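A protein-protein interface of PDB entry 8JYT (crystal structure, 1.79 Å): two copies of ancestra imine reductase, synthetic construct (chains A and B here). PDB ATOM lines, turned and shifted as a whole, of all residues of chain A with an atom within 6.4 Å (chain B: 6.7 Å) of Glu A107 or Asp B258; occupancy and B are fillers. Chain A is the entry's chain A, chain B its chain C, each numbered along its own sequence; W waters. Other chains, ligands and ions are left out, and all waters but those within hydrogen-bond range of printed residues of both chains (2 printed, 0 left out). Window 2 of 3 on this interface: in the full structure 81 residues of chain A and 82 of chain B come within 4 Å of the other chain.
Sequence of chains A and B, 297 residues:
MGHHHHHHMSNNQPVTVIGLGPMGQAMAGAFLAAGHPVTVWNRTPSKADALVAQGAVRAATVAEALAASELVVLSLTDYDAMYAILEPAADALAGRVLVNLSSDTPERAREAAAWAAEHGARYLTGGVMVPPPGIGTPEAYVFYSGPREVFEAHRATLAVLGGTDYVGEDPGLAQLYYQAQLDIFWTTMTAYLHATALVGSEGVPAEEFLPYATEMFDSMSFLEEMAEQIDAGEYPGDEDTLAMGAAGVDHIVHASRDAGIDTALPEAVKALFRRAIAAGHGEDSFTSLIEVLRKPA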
ATOM      1  N   ASP A 104      19.795  -4.104  18.509  1.00  0.00           N
ATOM      2  CA  ASP A 104      18.948  -2.937  18.255  1.00  0.00           C
ATOM      3  C   ASP A 104      17.650  -3.439  17.616  1.00  0.00           C
ATOM      4  O   ASP A 104      17.385  -4.648  17.584  1.00  0.00           O
ATOM      5  CB  ASP A 104      19.652  -1.904  17.368  1.00  0.00           C
ATOM      6  CG  ASP A 104      19.282  -0.483  17.746  1.00  0.00           C
ATOM      7  OD1 ASP A 104      18.089  -0.125  17.626  1.00  0.00           O
ATOM      8  OD2 ASP A 104      20.191   0.277  18.149  1.00  0.00           O
ATOM      9  N   THR A 105      16.821  -2.507  17.095  1.00  0.00           N
ATOM     10  CA  THR A 105      15.510  -2.937  16.636  1.00  0.00           C
ATOM     11  C   THR A 105      15.572  -3.403  15.189  1.00  0.00           C
ATOM     12  O   THR A 105      16.469  -3.008  14.422  1.00  0.00           O
ATOM     13  CB  THR A 105      14.487  -1.808  16.768  1.00  0.00           C
ATOM     14  OG1 THR A 105      14.870  -0.695  15.953  1.00  0.00           O
ATOM     15  CG2 THR A 105      14.375  -1.345  18.214  1.00  0.00           C
ATOM     16  N   PRO A 106      14.624  -4.257  14.789  1.00  0.00           N
ATOM     17  CA  PRO A 106      14.533  -4.608  13.369  1.00  0.00           C
ATOM     18  C   PRO A 106      14.422  -3.382  12.466  1.00  0.00           C
ATOM     19  O   PRO A 106      14.986  -3.376  11.365  1.00  0.00           O
ATOM     20  CB  PRO A 106      13.274  -5.482  13.307  1.00  0.00           C
ATOM     21  CG  PRO A 106      13.245  -6.186  14.656  1.00  0.00           C
ATOM     22  CD  PRO A 106      13.714  -5.075  15.629  1.00  0.00           C
ATOM     23  N   GLU A 107      13.711  -2.336  12.902  1.00  0.00           N
ATOM     24  CA  GLU A 107      13.569  -1.145  12.064  1.00  0.00           C
ATOM     25  C   GLU A 107      14.891  -0.392  11.931  1.00  0.00           C
ATOM     26  O   GLU A 107      15.219   0.118  10.850  1.00  0.00           O
ATOM     27  CB  GLU A 107      12.493  -0.242  12.656  1.00  0.00           C
ATOM     28  CG  GLU A 107      11.074  -0.603  12.200  1.00  0.00           C
ATOM     29  CD  GLU A 107      10.929  -0.595  10.678  1.00  0.00           C
ATOM     30  OE1 GLU A 107      11.313   0.407  10.049  1.00  0.00           O
ATOM     31  OE2 GLU A 107      10.449  -1.589  10.103  1.00  0.00           O
ATOM     32  N   ARG A 108      15.644  -0.278  13.030  1.00  0.00           N
ATOM     33  CA  ARG A 108      16.952   0.366  12.978  1.00  0.00           C
ATOM     34  C   ARG A 108      17.898  -0.416  12.097  1.00  0.00           C
ATOM     35  O   ARG A 108      18.775   0.178  11.460  1.00  0.00           O
ATOM     36  CB  ARG A 108      17.501   0.537  14.397  1.00  0.00           C
ATOM     37  CG  ARG A 108      16.745   1.649  15.134  1.00  0.00           C
ATOM     38  CD  ARG A 108      17.600   2.870  15.366  1.00  0.00           C
ATOM     39  NE  ARG A 108      18.613   2.599  16.383  1.00  0.00           N
ATOM     40  CZ  ARG A 108      19.273   3.534  17.057  1.00  0.00           C
ATOM     41  NH1 ARG A 108      19.179   4.817  16.736  1.00  0.00           N
ATOM     42  NH2 ARG A 108      20.068   3.172  18.059  1.00  0.00           N
ATOM     43  N   ALA A 109      17.723  -1.737  12.018  1.00  0.00           N
ATOM     44  CA  ALA A 109      18.535  -2.527  11.098  1.00  0.00           C
ATOM     45  C   ALA A 109      18.182  -2.208   9.651  1.00  0.00           C
ATOM     46  O   ALA A 109      19.066  -2.054   8.802  1.00  0.00           O
ATOM     47  CB  ALA A 109      18.351  -4.023  11.364  1.00  0.00           C
ATOM     48  N   ARG A 110      16.883  -2.131   9.348  1.00  0.00           N
ATOM     49  CA  ARG A 110      16.470  -1.819   7.984  1.00  0.00           C
ATOM     50  C   ARG A 110      16.970  -0.436   7.590  1.00  0.00           C
ATOM     51  O   ARG A 110      17.420  -0.230   6.460  1.00  0.00           O
ATOM     52  CB  ARG A 110      14.939  -1.871   7.840  1.00  0.00           C
ATOM     53  CG  ARG A 110      14.390  -3.268   8.025  1.00  0.00           C
ATOM     54  CD  ARG A 110      12.931  -3.260   8.564  1.00  0.00           C
ATOM     55  NE  ARG A 110      12.435  -4.629   8.634  1.00  0.00           N
ATOM     56  CZ  ARG A 110      11.593  -5.074   9.563  1.00  0.00           C
ATOM     57  NH1 ARG A 110      10.985  -4.253  10.404  1.00  0.00           N
ATOM     58  NH2 ARG A 110      11.368  -6.380   9.663  1.00  0.00           N
ATOM     59  N   GLU A 111      16.904   0.528   8.514  1.00  0.00           N
ATOM     60  CA  GLU A 111      17.382   1.881   8.237  1.00  0.00           C
ATOM     61  C   GLU A 111      18.880   1.878   7.950  1.00  0.00           C
ATOM     62  O   GLU A 111      19.349   2.486   6.979  1.00  0.00           O
ATOM     63  CB  GLU A 111      17.055   2.757   9.446  1.00  0.00           C
ATOM     64  CG  GLU A 111      18.029   3.870   9.723  1.00  0.00           C
ATOM     65  CD  GLU A 111      17.522   4.836  10.787  1.00  0.00           C
ATOM     66  OE1 GLU A 111      16.879   5.831  10.422  1.00  0.00           O
ATOM     67  OE2 GLU A 111      17.759   4.582  11.999  1.00  0.00           O
ATOM     68  N   ALA A 112      19.643   1.165   8.775  1.00  0.00           N
ATOM     69  CA  ALA A 112      21.090   1.142   8.602  1.00  0.00           C
ATOM     70  C   ALA A 112      21.467   0.484   7.288  1.00  0.00           C
ATOM     71  O   ALA A 112      22.421   0.903   6.624  1.00  0.00           O
ATOM     72  CB  ALA A 112      21.746   0.413   9.772  1.00  0.00           C
ATOM     73  N   GLY A 172      15.956  -6.679   8.882  1.00  0.00           N
ATOM     74  CA  GLY A 172      15.389  -6.684  10.219  1.00  0.00           C
ATOM     75  C   GLY A 172      15.222  -8.055  10.837  1.00  0.00           C
ATOM     76  O   GLY A 172      15.131  -8.156  12.060  1.00  0.00           O
ATOM     77  N   SER B 201       4.862 -11.317  13.229  1.00  0.00           N
ATOM     78  CA  SER B 201       4.551 -10.044  12.587  1.00  0.00           C
ATOM     79  C   SER B 201       5.226  -9.892  11.225  1.00  0.00           C
ATOM     80  O   SER B 201       4.853  -8.990  10.460  1.00  0.00           O
ATOM     81  CB  SER B 201       4.967  -8.883  13.499  1.00  0.00           C
ATOM     82  OG  SER B 201       6.377  -8.682  13.492  1.00  0.00           O
ATOM     83  N   GLU B 202       6.222 -10.728  10.917  1.00  0.00           N
ATOM     84  CA  GLU B 202       6.870 -10.731   9.611  1.00  0.00           C
ATOM     85  C   GLU B 202       6.631 -12.041   8.867  1.00  0.00           C
ATOM     86  O   GLU B 202       7.361 -12.363   7.924  1.00  0.00           O
ATOM     87  CB  GLU B 202       8.374 -10.484   9.753  1.00  0.00           C
ATOM     88  CG  GLU B 202       8.708  -9.058  10.197  1.00  0.00           C
ATOM     89  CD  GLU B 202       8.303  -8.010   9.191  1.00  0.00           C
ATOM     90  OE1 GLU B 202       8.235  -6.822   9.580  1.00  0.00           O
ATOM     91  OE2 GLU B 202       8.092  -8.357   8.008  1.00  0.00           O
ATOM     92  N   VAL B 253      10.687  -3.953  23.918  1.00  0.00           N
ATOM     93  CA  VAL B 253       9.539  -3.045  23.935  1.00  0.00           C
ATOM     94  C   VAL B 253       9.450  -2.281  22.618  1.00  0.00           C
ATOM     95  O   VAL B 253       8.383  -2.184  22.002  1.00  0.00           O
ATOM     96  CB  VAL B 253       9.633  -2.074  25.125  1.00  0.00           C
ATOM     97  CG1 VAL B 253       8.542  -1.000  25.015  1.00  0.00           C
ATOM     98  CG2 VAL B 253       9.557  -2.826  26.444  1.00  0.00           C
ATOM     99  N   HIS B 254      10.573  -1.700  22.178  1.00  0.00           N
ATOM    100  CA  HIS B 254      10.555  -0.899  20.959  1.00  0.00           C
ATOM    101  C   HIS B 254      10.267  -1.758  19.737  1.00  0.00           C
ATOM    102  O   HIS B 254       9.464  -1.367  18.879  1.00  0.00           O
ATOM    103  CB  HIS B 254      11.871  -0.139  20.824  1.00  0.00           C
ATOM    104  CG  HIS B 254      11.842   1.206  21.481  1.00  0.00           C
ATOM    105  ND1 HIS B 254      12.580   1.493  22.607  1.00  0.00           N
ATOM    106  CD2 HIS B 254      11.180   2.346  21.165  1.00  0.00           C
ATOM    107  CE1 HIS B 254      12.367   2.746  22.966  1.00  0.00           C
ATOM    108  NE2 HIS B 254      11.521   3.287  22.107  1.00  0.00           N
ATOM    109  N   ALA B 255      10.875  -2.943  19.656  1.00  0.00           N
ATOM    110  CA  ALA B 255      10.574  -3.836  18.541  1.00  0.00           C
ATOM    111  C   ALA B 255       9.099  -4.238  18.528  1.00  0.00           C
ATOM    112  O   ALA B 255       8.474  -4.309  17.460  1.00  0.00           O
ATOM    113  CB  ALA B 255      11.442  -5.082  18.620  1.00  0.00           C
ATOM    114  N   SER B 256       8.548  -4.546  19.700  1.00  0.00           N
ATOM    115  CA  SER B 256       7.136  -4.924  19.806  1.00  0.00           C
ATOM    116  C   SER B 256       6.221  -3.807  19.321  1.00  0.00           C
ATOM    117  O   SER B 256       5.280  -4.036  18.552  1.00  0.00           O
ATOM    118  CB  SER B 256       6.809  -5.274  21.256  1.00  0.00           C
ATOM    119  OG  SER B 256       7.541  -6.388  21.699  1.00  0.00           O
ATOM    120  N   ARG B 257       6.475  -2.588  19.782  1.00  0.00           N
ATOM    121  CA  ARG B 257       5.725  -1.432  19.305  1.00  0.00           C
ATOM    122  C   ARG B 257       5.798  -1.317  17.781  1.00  0.00           C
ATOM    123  O   ARG B 257       4.769  -1.230  17.098  1.00  0.00           O
ATOM    124  CB  ARG B 257       6.279  -0.174  19.980  1.00  0.00           C
ATOM    125  CG  ARG B 257       5.226   0.887  20.283  1.00  0.00           C
ATOM    126  CD  ARG B 257       5.469   1.457  21.692  1.00  0.00           C
ATOM    127  NE  ARG B 257       6.888   1.611  22.007  1.00  0.00           N
ATOM    128  CZ  ARG B 257       7.378   1.882  23.211  1.00  0.00           C
ATOM    129  NH1 ARG B 257       6.607   1.929  24.279  1.00  0.00           N
ATOM    130  NH2 ARG B 257       8.675   2.137  23.344  1.00  0.00           N
ATOM    131  N   ASP B 258       7.017  -1.242  17.233  1.00  0.00           N
ATOM    132  CA  ASP B 258       7.209  -1.150  15.788  1.00  0.00           C
ATOM    133  C   ASP B 258       6.466  -2.246  15.038  1.00  0.00           C
ATOM    134  O   ASP B 258       6.006  -2.037  13.908  1.00  0.00           O
ATOM    135  CB  ASP B 258       8.712  -1.241  15.468  1.00  0.00           C
ATOM    136  CG  ASP B 258       9.515  -0.046  15.952  1.00  0.00           C
ATOM    137  OD1 ASP B 258       8.939   0.963  16.378  1.00  0.00           O
ATOM    138  OD2 ASP B 258      10.755  -0.111  15.900  1.00  0.00           O
ATOM    139  N   ALA B 259       6.406  -3.440  15.613  1.00  0.00           N
ATOM    140  CA  ALA B 259       5.788  -4.566  14.925  1.00  0.00           C
ATOM    141  C   ALA B 259       4.262  -4.544  14.985  1.00  0.00           C
ATOM    142  O   ALA B 259       3.615  -5.390  14.352  1.00  0.00           O
ATOM    143  CB  ALA B 259       6.297  -5.882  15.520  1.00  0.00           C
ATOM    144  N   GLY B 260       3.681  -3.635  15.758  1.00  0.00           N
ATOM    145  CA  GLY B 260       2.240  -3.599  15.912  1.00  0.00           C
ATOM    146  C   GLY B 260       1.645  -4.650  16.818  1.00  0.00           C
ATOM    147  O   GLY B 260       0.445  -4.917  16.723  1.00  0.00           O
ATOM    148  N   ILE B 261       2.433  -5.234  17.717  1.00  0.00           N
ATOM    149  CA  ILE B 261       1.918  -6.226  18.649  1.00  0.00           C
ATOM    150  C   ILE B 261       1.766  -5.569  20.011  1.00  0.00           C
ATOM    151  O   ILE B 261       2.124  -4.402  20.196  1.00  0.00           O
ATOM    152  CB  ILE B 261       2.819  -7.473  18.707  1.00  0.00           C
ATOM    153  CG1 ILE B 261       4.170  -7.151  19.345  1.00  0.00           C
ATOM    154  CG2 ILE B 261       3.005  -8.061  17.321  1.00  0.00           C
ATOM    155  CD1 ILE B 261       4.877  -8.403  19.896  1.00  0.00           C
ATOM    156  N   THR B 263       2.379  -4.385  23.770  1.00  0.00           N
ATOM    157  CA  THR B 263       3.575  -4.006  24.499  1.00  0.00           C
ATOM    158  C   THR B 263       3.392  -4.102  26.001  1.00  0.00           C
ATOM    159  O   THR B 263       4.333  -3.804  26.746  1.00  0.00           O
ATOM    160  CB  THR B 263       3.998  -2.573  24.147  1.00  0.00           C
ATOM    161  OG1 THR B 263       2.908  -1.670  24.387  1.00  0.00           O
ATOM    162  CG2 THR B 263       4.389  -2.482  22.694  1.00  0.00           C
HETATM  163  O   HOH W   1      11.728  -2.669  15.073  1.00  0.00           O
HETATM  164  O   HOH W   2      13.005   1.177  16.125  1.00  0.00           O
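The side-chain carboxylate of Glu B202 lies within salt-bridge range of the guanidinium group of Arg A110 (3.2 Å).
The side-chain carboxylate (OE2) of Glu A107 is in salt-bridge range of the guanidinium group (NH1) of Arg A110.
N of Arg A108 lies within hydrogen-bond range of OG1 of Thr A105 (3.1 Å).
A ring nitrogen (NE2) of His B254 is in hydrogen-bond range of the guanidinium group (NH2) of Arg B257, at 3.3 Å.
Among the printed residues, pairs that only touch across the chains: Glu A107 with Asp B258 (3.7 Å), Pro A106 with Ala B255 (3.8 Å) and Thr A105 with His B254 (3.8 Å).
Glu A107 touches just one residue of chain B: Asp B258.
Of chain A, only Glu A107 comes within 4 Å of Asp B258.
Printed residues of chain B within 4 Å of Pro A106: Ala B255 (3.8 Å).
Of the printed residues of chain B, Arg A110 touches Glu B202 (3.2 Å).
Thr B263 touches none of the printed residues of chain A.
Gly A172 touches none of the printed residues of chain B.
The nearest residue of chain A that does not touch Asp B258 is Thr A105 (4.2 Å).
Hydrophobic or aromatic side chains of chain B that line the printed part of chain A: His B254 and Ala B255.
Of the 10 printed residues of chain A, 4 touch a printed residue of chain B.
Hydrophobic or aromatic side chains of chain A that line the printed part of chain B: Pro A106.
No position is printed for both chains.
Water W2 lies within hydrogen-bond range of the side-chain carboxylate of Asp B258 and the side-chain hydroxyl of Thr A105.
Water W1 bridges OD2 of Asp B258 (2.9 Å) and N of Glu A107 (3.0 Å).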
